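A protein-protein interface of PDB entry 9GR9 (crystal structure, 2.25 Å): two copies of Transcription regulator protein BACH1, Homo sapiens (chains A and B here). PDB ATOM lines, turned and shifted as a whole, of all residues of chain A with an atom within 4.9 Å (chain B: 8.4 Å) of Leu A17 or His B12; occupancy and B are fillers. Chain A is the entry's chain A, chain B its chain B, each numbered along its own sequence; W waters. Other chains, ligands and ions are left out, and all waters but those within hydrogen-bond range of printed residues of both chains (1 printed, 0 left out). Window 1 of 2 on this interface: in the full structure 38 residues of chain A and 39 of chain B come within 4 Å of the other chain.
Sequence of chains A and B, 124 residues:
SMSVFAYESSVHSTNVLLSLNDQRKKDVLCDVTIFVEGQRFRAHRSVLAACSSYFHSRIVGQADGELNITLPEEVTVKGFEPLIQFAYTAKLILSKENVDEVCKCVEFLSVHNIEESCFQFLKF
OG of Ser B13 is in hydrogen-bond range of OG of Ser A13, at 2.8 Å. ND1 of His B12 sits at hydrogen-bond distance from ND2 of Asn A113 (3.3 Å). The backbone carbonyl oxygen (O) of Ala A87 lies within hydrogen-bond range of a ring nitrogen (NE2) of His B12 (3.0 Å). The backbone NH (N) of Ser B9 is in hydrogen-bond range of the backbone carbonyl oxygen (O) of Ala A90, at 3.2 Å. O of Asn A113 lies within hydrogen-bond range of OH of Tyr B7 (3.2 Å).
O of Cys A51 sits at hydrogen-bond distance from N of His A112. The side-chain hydroxyl (OG) of Ser B19 sits at hydrogen-bond distance from the backbone carbonyl oxygen (O) of Asn B15, at 2.8 Å. The backbone NH of Val B11 lies close to the side-chain hydroxyl of Ser B9 (3.3 Å). N of His B12 lies within hydrogen-bond range of OG of Ser B9 (3.1 Å). The backbone carbonyl oxygen (O) of Asn A15 sits at hydrogen-bond distance from the side-chain hydroxyl (OG) of Ser A19, 3.0 Å away. The backbone carbonyl oxygen (O) of Val B11 lies within hydrogen-bond range of the side-chain amide nitrogen (ND2) of Asn B15 (2.8 Å).
Among the printed residues, pairs that only touch across the chains: Ala A90 with Glu B8 (3.5 Å), Phe A86 with His B12 (3.5 Å), Thr A14 with Ser B13 (3.5 Å), Ser A19 with Ala B50 (3.5 Å), Cys A51 with His B12 (3.6 Å), Phe A86 with Tyr B7 (3.6 Å), Asn A113 with Ser B9 (3.7 Å), Asn A113 with Asn B15 (3.8 Å), Ala A90 with His B12 (3.8 Å), Leu A17 with His B12 (3.8 Å), Ser A13 with Thr B14 (3.8 Å), Ser A13 with Leu B17 (3.9 Å), Ala A90 with Tyr B7 (3.96 Å), Cys A51 with Val B16 (3.97 Å) and Asn A113 with Val B11 (3.99 Å).
Of the printed residues of chain B, Leu A17 touches His B12 (3.8 Å). Of the printed residues of chain A, Asn B15 touches Asn A113. Of the printed residues of chain A, Ala B50 touches Ser A19 (3.5 Å). Of the printed residues of chain A, Val B11 touches Asn A113. Val B47 touches none of the printed residues of chain A. Thr A89 touches none of the printed residues of chain B. The nearest printed residue of chain B that does not touch Leu A17 is Ser B13 (4.01 Å). The nearest residue of chain A that does not touch His B12 is His A112 (4.4 Å). The nearest printed residue of chain A that does not touch Ser B13 is Leu A17 (4.01 Å).
Printed residues of chain B that touch a printed residue of chain A: Tyr B7, Glu B8, Ser B9, Val B11, His B12, Ser B13, Thr B14, Asn B15, Val B16, Leu B17 and Ala B50. Hydrophobic or aromatic side chains of chain B that line the printed part of chain A: Tyr B7, Val B11, His B12, Val B16, Leu B17 and Ala B50. Printed residues of chain A that touch a printed residue of chain B: Ser A13, Thr A14, Leu A17, Ser A19, Cys A51, Phe A86, Ala A87, Ala A90 and Asn A113.
Ser B13 touches its own counterpart, Ser A13. Ser A13 touches Thr B14, and with the chains exchanged Thr A14 touches Ser B13. Ser A13 touches Leu B17, but with the chains exchanged Leu A17 does not touch Ser B13 (4.01 Å). Cys A51 touches Val B16, but with the chains exchanged Val A16 does not touch Cys B51 (4.1 Å). Of the 20 pairs that touch across the chains among the printed residues, 3 have their exchanged pair printed and touching as well.
Water W1 lies within hydrogen-bond range of OG1 of Thr A14 (2.9 Å) and OG of Ser B13 (3.4 Å).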
ATOM      1  N   SER A  13      26.899 -21.810 -23.275  1.00  0.00           N
ATOM      2  CA  SER A  13      27.383 -23.101 -23.755  1.00  0.00           C
ATOM      3  C   SER A  13      26.601 -24.245 -23.122  1.00  0.00           C
ATOM      4  O   SER A  13      26.312 -25.251 -23.779  1.00  0.00           O
ATOM      5  CB  SER A  13      28.876 -23.240 -23.462  1.00  0.00           C
ATOM      6  OG  SER A  13      29.114 -23.270 -22.068  1.00  0.00           O
ATOM      7  N   THR A  14      26.235 -24.100 -21.847  1.00  0.00           N
ATOM      8  CA  THR A  14      25.388 -25.096 -21.201  1.00  0.00           C
ATOM      9  C   THR A  14      23.988 -25.106 -21.804  1.00  0.00           C
ATOM     10  O   THR A  14      23.377 -26.170 -21.953  1.00  0.00           O
ATOM     11  CB  THR A  14      25.323 -24.829 -19.697  1.00  0.00           C
ATOM     12  OG1 THR A  14      26.653 -24.769 -19.166  1.00  0.00           O
ATOM     13  CG2 THR A  14      24.548 -25.933 -18.993  1.00  0.00           C
ATOM     14  N   ASN A  15      23.465 -23.930 -22.160  1.00  0.00           N
ATOM     15  CA  ASN A  15      22.123 -23.858 -22.730  1.00  0.00           C
ATOM     16  C   ASN A  15      22.052 -24.563 -24.078  1.00  0.00           C
ATOM     17  O   ASN A  15      21.092 -25.293 -24.354  1.00  0.00           O
ATOM     18  CB  ASN A  15      21.685 -22.399 -22.865  1.00  0.00           C
ATOM     19  CG  ASN A  15      21.359 -21.762 -21.529  1.00  0.00           C
ATOM     20  OD1 ASN A  15      20.896 -22.432 -20.607  1.00  0.00           O
ATOM     21  ND2 ASN A  15      21.601 -20.461 -21.418  1.00  0.00           N
ATOM     22  N   VAL A  16      23.058 -24.358 -24.933  1.00  0.00           N
ATOM     23  CA  VAL A  16      23.071 -25.007 -26.243  1.00  0.00           C
ATOM     24  C   VAL A  16      23.168 -26.519 -26.083  1.00  0.00           C
ATOM     25  O   VAL A  16      22.432 -27.280 -26.724  1.00  0.00           O
ATOM     26  CB  VAL A  16      24.223 -24.460 -27.104  1.00  0.00           C
ATOM     27  CG1 VAL A  16      24.230 -25.128 -28.473  1.00  0.00           C
ATOM     28  CG2 VAL A  16      24.118 -22.947 -27.242  1.00  0.00           C
ATOM     29  N   LEU A  17      24.076 -26.976 -25.218  1.00  0.00           N
ATOM     30  CA  LEU A  17      24.274 -28.409 -25.030  1.00  0.00           C
ATOM     31  C   LEU A  17      23.011 -29.077 -24.497  1.00  0.00           C
ATOM     32  O   LEU A  17      22.695 -30.211 -24.874  1.00  0.00           O
ATOM     33  CB  LEU A  17      25.454 -28.650 -24.089  1.00  0.00           C
ATOM     34  CG  LEU A  17      26.012 -30.070 -24.017  1.00  0.00           C
ATOM     35  CD1 LEU A  17      26.548 -30.490 -25.375  1.00  0.00           C
ATOM     36  CD2 LEU A  17      27.098 -30.164 -22.957  1.00  0.00           C
ATOM     37  N   LEU A  18      22.270 -28.387 -23.626  1.00  0.00           N
ATOM     38  CA  LEU A  18      21.021 -28.944 -23.114  1.00  0.00           C
ATOM     39  C   LEU A  18      19.914 -28.907 -24.162  1.00  0.00           C
ATOM     40  O   LEU A  18      18.985 -29.721 -24.109  1.00  0.00           O
ATOM     41  CB  LEU A  18      20.588 -28.197 -21.852  1.00  0.00           C
ATOM     42  CG  LEU A  18      21.047 -28.778 -20.509  1.00  0.00           C
ATOM     43  CD1 LEU A  18      22.565 -28.935 -20.445  1.00  0.00           C
ATOM     44  CD2 LEU A  18      20.542 -27.916 -19.357  1.00  0.00           C
ATOM     45  N   SER A  19      19.990 -27.973 -25.113  1.00  0.00           N
ATOM     46  CA  SER A  19      19.027 -27.961 -26.209  1.00  0.00           C
ATOM     47  C   SER A  19      19.336 -29.054 -27.224  1.00  0.00           C
ATOM     48  O   SER A  19      18.418 -29.681 -27.768  1.00  0.00           O
ATOM     49  CB  SER A  19      19.015 -26.591 -26.883  1.00  0.00           C
ATOM     50  OG  SER A  19      18.623 -25.577 -25.973  1.00  0.00           O
ATOM     51  N   LEU A  20      20.623 -29.293 -27.494  1.00  0.00           N
ATOM     52  CA  LEU A  20      21.004 -30.396 -28.370  1.00  0.00           C
ATOM     53  C   LEU A  20      20.621 -31.739 -27.761  1.00  0.00           C
ATOM     54  O   LEU A  20      20.192 -32.655 -28.475  1.00  0.00           O
ATOM     55  CB  LEU A  20      22.506 -30.346 -28.650  1.00  0.00           C
ATOM     56  CG  LEU A  20      23.043 -29.093 -29.345  1.00  0.00           C
ATOM     57  CD1 LEU A  20      24.554 -29.124 -29.396  1.00  0.00           C
ATOM     58  CD2 LEU A  20      22.477 -28.973 -30.743  1.00  0.00           C
ATOM     59  N   ASN A  21      20.772 -31.877 -26.441  1.00  0.00           N
ATOM     60  CA  ASN A  21      20.365 -33.110 -25.777  1.00  0.00           C
ATOM     61  C   ASN A  21      18.858 -33.310 -25.846  1.00  0.00           C
ATOM     62  O   ASN A  21      18.388 -34.452 -25.923  1.00  0.00           O
ATOM     63  CB  ASN A  21      20.829 -33.098 -24.322  1.00  0.00           C
ATOM     64  CG  ASN A  21      20.637 -34.434 -23.642  1.00  0.00           C
ATOM     65  OD1 ASN A  21      20.793 -35.487 -24.262  1.00  0.00           O
ATOM     66  ND2 ASN A  21      20.290 -34.402 -22.362  1.00  0.00           N
ATOM     67  N   CYS A  51      33.491 -34.719 -29.251  1.00  0.00           N
ATOM     68  CA  CYS A  51      33.650 -35.385 -27.968  1.00  0.00           C
ATOM     69  C   CYS A  51      34.462 -36.668 -28.032  1.00  0.00           C
ATOM     70  O   CYS A  51      34.801 -37.211 -26.974  1.00  0.00           O
ATOM     71  CB  CYS A  51      32.275 -35.707 -27.363  1.00  0.00           C
ATOM     72  SG  CYS A  51      31.242 -34.261 -27.087  1.00  0.00           S
ATOM     73  N   PHE A  86      26.877 -38.068 -21.009  1.00  0.00           N
ATOM     74  CA  PHE A  86      27.879 -37.079 -20.624  1.00  0.00           C
ATOM     75  C   PHE A  86      28.174 -36.109 -21.760  1.00  0.00           C
ATOM     76  O   PHE A  86      28.305 -34.900 -21.533  1.00  0.00           O
ATOM     77  CB  PHE A  86      29.162 -37.783 -20.175  1.00  0.00           C
ATOM     78  CG  PHE A  86      30.330 -36.854 -19.989  1.00  0.00           C
ATOM     79  CD1 PHE A  86      30.509 -36.176 -18.796  1.00  0.00           C
ATOM     80  CD2 PHE A  86      31.249 -36.658 -21.009  1.00  0.00           C
ATOM     81  CE1 PHE A  86      31.580 -35.319 -18.623  1.00  0.00           C
ATOM     82  CE2 PHE A  86      32.319 -35.802 -20.842  1.00  0.00           C
ATOM     83  CZ  PHE A  86      32.486 -35.133 -19.648  1.00  0.00           C
ATOM     84  N   ALA A  87      28.289 -36.619 -22.990  1.00  0.00           N
ATOM     85  CA  ALA A  87      28.604 -35.757 -24.125  1.00  0.00           C
ATOM     86  C   ALA A  87      27.553 -34.675 -24.325  1.00  0.00           C
ATOM     87  O   ALA A  87      27.865 -33.594 -24.840  1.00  0.00           O
ATOM     88  CB  ALA A  87      28.744 -36.594 -25.397  1.00  0.00           C
ATOM     89  N   TYR A  88      26.312 -34.936 -23.918  1.00  0.00           N
ATOM     90  CA  TYR A  88      25.214 -33.999 -24.101  1.00  0.00           C
ATOM     91  C   TYR A  88      24.801 -33.294 -22.814  1.00  0.00           C
ATOM     92  O   TYR A  88      23.979 -32.375 -22.866  1.00  0.00           O
ATOM     93  CB  TYR A  88      24.010 -34.726 -24.710  1.00  0.00           C
ATOM     94  CG  TYR A  88      24.111 -34.937 -26.207  1.00  0.00           C
ATOM     95  CD1 TYR A  88      23.602 -33.996 -27.093  1.00  0.00           C
ATOM     96  CD2 TYR A  88      24.717 -36.071 -26.734  1.00  0.00           C
ATOM     97  CE1 TYR A  88      23.689 -34.177 -28.461  1.00  0.00           C
ATOM     98  CE2 TYR A  88      24.810 -36.260 -28.107  1.00  0.00           C
ATOM     99  CZ  TYR A  88      24.293 -35.310 -28.964  1.00  0.00           C
ATOM    100  OH  TYR A  88      24.376 -35.483 -30.328  1.00  0.00           O
ATOM    101  N   THR A  89      25.347 -33.696 -21.662  1.00  0.00           N
ATOM    102  CA  THR A  89      24.992 -33.083 -20.387  1.00  0.00           C
ATOM    103  C   THR A  89      26.186 -32.655 -19.546  1.00  0.00           C
ATOM    104  O   THR A  89      25.979 -31.994 -18.523  1.00  0.00           O
ATOM    105  CB  THR A  89      24.132 -34.037 -19.536  1.00  0.00           C
ATOM    106  OG1 THR A  89      24.935 -35.131 -19.076  1.00  0.00           O
ATOM    107  CG2 THR A  89      22.952 -34.577 -20.334  1.00  0.00           C
ATOM    108  N   ALA A  90      27.413 -33.014 -19.930  1.00  0.00           N
ATOM    109  CA  ALA A  90      28.618 -32.779 -19.136  1.00  0.00           C
ATOM    110  C   ALA A  90      28.538 -33.427 -17.757  1.00  0.00           C
ATOM    111  O   ALA A  90      29.258 -33.027 -16.836  1.00  0.00           O
ATOM    112  CB  ALA A  90      28.919 -31.279 -19.001  1.00  0.00           C
ATOM    113  N   HIS A 112      36.564 -37.200 -24.542  1.00  0.00           N
ATOM    114  CA  HIS A 112      37.304 -36.088 -23.968  1.00  0.00           C
ATOM    115  C   HIS A 112      36.639 -35.572 -22.695  1.00  0.00           C
ATOM    116  O   HIS A 112      35.454 -35.805 -22.441  1.00  0.00           O
ATOM    117  CB  HIS A 112      37.424 -34.950 -24.982  1.00  0.00           C
ATOM    118  CG  HIS A 112      38.017 -35.366 -26.292  1.00  0.00           C
ATOM    119  ND1 HIS A 112      39.078 -36.239 -26.387  1.00  0.00           N
ATOM    120  CD2 HIS A 112      37.692 -35.029 -27.563  1.00  0.00           C
ATOM    121  CE1 HIS A 112      39.383 -36.421 -27.659  1.00  0.00           C
ATOM    122  NE2 HIS A 112      38.557 -35.697 -28.393  1.00  0.00           N
ATOM    123  N   ASN A 113      37.438 -34.871 -21.887  1.00  0.00           N
ATOM    124  CA  ASN A 113      36.963 -34.074 -20.755  1.00  0.00           C
ATOM    125  C   ASN A 113      36.405 -34.926 -19.617  1.00  0.00           C
ATOM    126  O   ASN A 113      35.516 -34.483 -18.887  1.00  0.00           O
ATOM    127  CB  ASN A 113      35.918 -33.048 -21.201  1.00  0.00           C
ATOM    128  CG  ASN A 113      36.445 -32.109 -22.262  1.00  0.00           C
ATOM    129  OD1 ASN A 113      37.576 -31.628 -22.176  1.00  0.00           O
ATOM    130  ND2 ASN A 113      35.631 -31.847 -23.278  1.00  0.00           N
ATOM    131  N   TYR B   7      29.892 -37.288 -11.645  1.00  0.00           N
ATOM    132  CA  TYR B   7      30.958 -36.425 -12.134  1.00  0.00           C
ATOM    133  C   TYR B   7      30.385 -35.300 -12.987  1.00  0.00           C
ATOM    134  O   TYR B   7      29.437 -35.503 -13.750  1.00  0.00           O
ATOM    135  CB  TYR B   7      31.973 -37.236 -12.943  1.00  0.00           C
ATOM    136  CG  TYR B   7      32.992 -36.395 -13.684  1.00  0.00           C
ATOM    137  CD1 TYR B   7      34.127 -35.916 -13.042  1.00  0.00           C
ATOM    138  CD2 TYR B   7      32.822 -36.088 -15.029  1.00  0.00           C
ATOM    139  CE1 TYR B   7      35.060 -35.144 -13.718  1.00  0.00           C
ATOM    140  CE2 TYR B   7      33.748 -35.317 -15.712  1.00  0.00           C
ATOM    141  CZ  TYR B   7      34.865 -34.849 -15.052  1.00  0.00           C
ATOM    142  OH  TYR B   7      35.785 -34.085 -15.732  1.00  0.00           O
ATOM    143  N   GLU B   8      30.964 -34.109 -12.847  1.00  0.00           N
ATOM    144  CA  GLU B   8      30.580 -32.947 -13.639  1.00  0.00           C
ATOM    145  C   GLU B   8      31.833 -32.241 -14.132  1.00  0.00           C
ATOM    146  O   GLU B   8      32.749 -31.972 -13.348  1.00  0.00           O
ATOM    147  CB  GLU B   8      29.717 -31.968 -12.835  1.00  0.00           C
ATOM    148  CG  GLU B   8      28.294 -32.434 -12.579  1.00  0.00           C
ATOM    149  CD  GLU B   8      27.323 -31.275 -12.419  1.00  0.00           C
ATOM    150  OE1 GLU B   8      27.462 -30.271 -13.152  1.00  0.00           O
ATOM    151  OE2 GLU B   8      26.422 -31.364 -11.557  1.00  0.00           O
ATOM    152  N   SER B   9      31.869 -31.945 -15.427  1.00  0.00           N
ATOM    153  CA  SER B   9      32.960 -31.198 -16.036  1.00  0.00           C
ATOM    154  C   SER B   9      32.531 -29.754 -16.249  1.00  0.00           C
ATOM    155  O   SER B   9      31.505 -29.494 -16.887  1.00  0.00           O
ATOM    156  CB  SER B   9      33.378 -31.823 -17.368  1.00  0.00           C
ATOM    157  OG  SER B   9      34.292 -30.988 -18.054  1.00  0.00           O
ATOM    158  N   SER B  10      33.312 -28.819 -15.712  1.00  0.00           N
ATOM    159  CA  SER B  10      33.051 -27.402 -15.927  1.00  0.00           C
ATOM    160  C   SER B  10      33.578 -26.904 -17.266  1.00  0.00           C
ATOM    161  O   SER B  10      33.273 -25.769 -17.649  1.00  0.00           O
ATOM    162  CB  SER B  10      33.664 -26.575 -14.794  1.00  0.00           C
ATOM    163  OG  SER B  10      35.073 -26.714 -14.768  1.00  0.00           O
ATOM    164  N   VAL B  11      34.347 -27.721 -17.983  1.00  0.00           N
ATOM    165  CA  VAL B  11      34.955 -27.315 -19.246  1.00  0.00           C
ATOM    166  C   VAL B  11      34.343 -28.007 -20.452  1.00  0.00           C
ATOM    167  O   VAL B  11      34.696 -27.656 -21.590  1.00  0.00           O
ATOM    168  CB  VAL B  11      36.480 -27.553 -19.236  1.00  0.00           C
ATOM    169  CG1 VAL B  11      37.118 -26.876 -18.034  1.00  0.00           C
ATOM    170  CG2 VAL B  11      36.775 -29.046 -19.241  1.00  0.00           C
ATOM    171  N   HIS B  12      33.447 -28.976 -20.254  1.00  0.00           N
ATOM    172  CA  HIS B  12      32.958 -29.763 -21.382  1.00  0.00           C
ATOM    173  C   HIS B  12      32.067 -28.933 -22.298  1.00  0.00           C
ATOM    174  O   HIS B  12      32.283 -28.889 -23.514  1.00  0.00           O
ATOM    175  CB  HIS B  12      32.209 -31.000 -20.886  1.00  0.00           C
ATOM    176  CG  HIS B  12      31.646 -31.838 -21.991  1.00  0.00           C
ATOM    177  ND1 HIS B  12      32.434 -32.623 -22.803  1.00  0.00           N
ATOM    178  CD2 HIS B  12      30.374 -32.002 -22.426  1.00  0.00           C
ATOM    179  CE1 HIS B  12      31.671 -33.240 -23.689  1.00  0.00           C
ATOM    180  NE2 HIS B  12      30.418 -32.880 -23.482  1.00  0.00           N
ATOM    181  N   SER B  13      31.052 -28.271 -21.732  1.00  0.00           N
ATOM    182  CA  SER B  13      30.132 -27.490 -22.554  1.00  0.00           C
ATOM    183  C   SER B  13      30.857 -26.388 -23.315  1.00  0.00           C
ATOM    184  O   SER B  13      30.468 -26.049 -24.439  1.00  0.00           O
ATOM    185  CB  SER B  13      29.029 -26.894 -21.684  1.00  0.00           C
ATOM    186  OG  SER B  13      29.507 -25.767 -20.972  1.00  0.00           O
ATOM    187  N   THR B  14      31.913 -25.824 -22.727  1.00  0.00           N
ATOM    188  CA  THR B  14      32.686 -24.799 -23.419  1.00  0.00           C
ATOM    189  C   THR B  14      33.461 -25.385 -24.595  1.00  0.00           C
ATOM    190  O   THR B  14      33.508 -24.784 -25.675  1.00  0.00           O
ATOM    191  CB  THR B  14      33.637 -24.113 -22.439  1.00  0.00           C
ATOM    192  OG1 THR B  14      32.887 -23.564 -21.348  1.00  0.00           O
ATOM    193  CG2 THR B  14      34.402 -22.998 -23.133  1.00  0.00           C
ATOM    194  N   ASN B  15      34.069 -26.559 -24.408  1.00  0.00           N
ATOM    195  CA  ASN B  15      34.869 -27.158 -25.473  1.00  0.00           C
ATOM    196  C   ASN B  15      34.001 -27.622 -26.635  1.00  0.00           C
ATOM    197  O   ASN B  15      34.417 -27.541 -27.797  1.00  0.00           O
ATOM    198  CB  ASN B  15      35.695 -28.322 -24.923  1.00  0.00           C
ATOM    199  CG  ASN B  15      36.996 -27.867 -24.292  1.00  0.00           C
ATOM    200  OD1 ASN B  15      37.920 -27.445 -24.989  1.00  0.00           O
ATOM    201  ND2 ASN B  15      37.079 -27.959 -22.970  1.00  0.00           N
ATOM    202  N   VAL B  16      32.797 -28.119 -26.346  1.00  0.00           N
ATOM    203  CA  VAL B  16      31.884 -28.517 -27.415  1.00  0.00           C
ATOM    204  C   VAL B  16      31.520 -27.311 -28.271  1.00  0.00           C
ATOM    205  O   VAL B  16      31.532 -27.375 -29.506  1.00  0.00           O
ATOM    206  CB  VAL B  16      30.631 -29.192 -26.829  1.00  0.00           C
ATOM    207  CG1 VAL B  16      29.653 -29.539 -27.938  1.00  0.00           C
ATOM    208  CG2 VAL B  16      31.015 -30.438 -26.051  1.00  0.00           C
ATOM    209  N   LEU B  17      31.203 -26.189 -27.624  1.00  0.00           N
ATOM    210  CA  LEU B  17      30.873 -24.975 -28.359  1.00  0.00           C
ATOM    211  C   LEU B  17      32.084 -24.444 -29.118  1.00  0.00           C
ATOM    212  O   LEU B  17      31.948 -23.923 -30.232  1.00  0.00           O
ATOM    213  CB  LEU B  17      30.331 -23.918 -27.399  1.00  0.00           C
ATOM    214  CG  LEU B  17      29.743 -22.659 -28.037  1.00  0.00           C
ATOM    215  CD1 LEU B  17      28.560 -23.021 -28.924  1.00  0.00           C
ATOM    216  CD2 LEU B  17      29.335 -21.656 -26.968  1.00  0.00           C
ATOM    217  N   LEU B  18      33.278 -24.569 -28.531  1.00  0.00           N
ATOM    218  CA  LEU B  18      34.493 -24.172 -29.236  1.00  0.00           C
ATOM    219  C   LEU B  18      34.709 -25.022 -30.479  1.00  0.00           C
ATOM    220  O   LEU B  18      35.097 -24.507 -31.534  1.00  0.00           O
ATOM    221  CB  LEU B  18      35.702 -24.275 -28.308  1.00  0.00           C
ATOM    222  CG  LEU B  18      35.905 -23.151 -27.290  1.00  0.00           C
ATOM    223  CD1 LEU B  18      37.102 -23.457 -26.411  1.00  0.00           C
ATOM    224  CD2 LEU B  18      36.087 -21.817 -27.996  1.00  0.00           C
ATOM    225  N   SER B  19      34.465 -26.329 -30.375  1.00  0.00           N
ATOM    226  CA  SER B  19      34.608 -27.200 -31.535  1.00  0.00           C
ATOM    227  C   SER B  19      33.552 -26.892 -32.589  1.00  0.00           C
ATOM    228  O   SER B  19      33.840 -26.923 -33.791  1.00  0.00           O
ATOM    229  CB  SER B  19      34.526 -28.663 -31.103  1.00  0.00           C
ATOM    230  OG  SER B  19      35.396 -28.925 -30.015  1.00  0.00           O
ATOM    231  N   LEU B  20      32.325 -26.588 -32.157  1.00  0.00           N
ATOM    232  CA  LEU B  20      31.272 -26.234 -33.105  1.00  0.00           C
ATOM    233  C   LEU B  20      31.619 -24.960 -33.865  1.00  0.00           C
ATOM    234  O   LEU B  20      31.414 -24.879 -35.083  1.00  0.00           O
ATOM    235  CB  LEU B  20      29.939 -26.073 -32.373  1.00  0.00           C
ATOM    236  CG  LEU B  20      29.288 -27.353 -31.844  1.00  0.00           C
ATOM    237  CD1 LEU B  20      28.103 -27.026 -30.961  1.00  0.00           C
ATOM    238  CD2 LEU B  20      28.857 -28.238 -32.995  1.00  0.00           C
ATOM    239  N   VAL B  47      22.233 -26.138 -33.967  1.00  0.00           N
ATOM    240  CA  VAL B  47      22.641 -25.028 -33.111  1.00  0.00           C
ATOM    241  C   VAL B  47      21.735 -23.823 -33.327  1.00  0.00           C
ATOM    242  O   VAL B  47      21.332 -23.152 -32.368  1.00  0.00           O
ATOM    243  CB  VAL B  47      24.122 -24.681 -33.358  1.00  0.00           C
ATOM    244  CG1 VAL B  47      24.534 -23.476 -32.527  1.00  0.00           C
ATOM    245  CG2 VAL B  47      25.015 -25.876 -33.042  1.00  0.00           C
ATOM    246  N   ALA B  50      18.571 -24.311 -31.659  1.00  0.00           N
ATOM    247  CA  ALA B  50      18.722 -24.201 -30.213  1.00  0.00           C
ATOM    248  C   ALA B  50      18.636 -22.750 -29.759  1.00  0.00           C
ATOM    249  O   ALA B  50      18.047 -22.455 -28.713  1.00  0.00           O
ATOM    250  CB  ALA B  50      20.051 -24.820 -29.778  1.00  0.00           C
ATOM    251  N   CYS B  51      19.202 -21.831 -30.539  1.00  0.00           N
ATOM    252  CA  CYS B  51      19.327 -20.438 -30.133  1.00  0.00           C
ATOM    253  C   CYS B  51      18.202 -19.548 -30.642  1.00  0.00           C
ATOM    254  O   CYS B  51      18.131 -18.383 -30.236  1.00  0.00           O
ATOM    255  CB  CYS B  51      20.667 -19.870 -30.616  1.00  0.00           C
ATOM    256  SG  CYS B  51      22.106 -20.857 -30.156  1.00  0.00           S
HETATM  257  O   HOH W   1      27.807 -27.383 -18.566  1.00  0.00           O
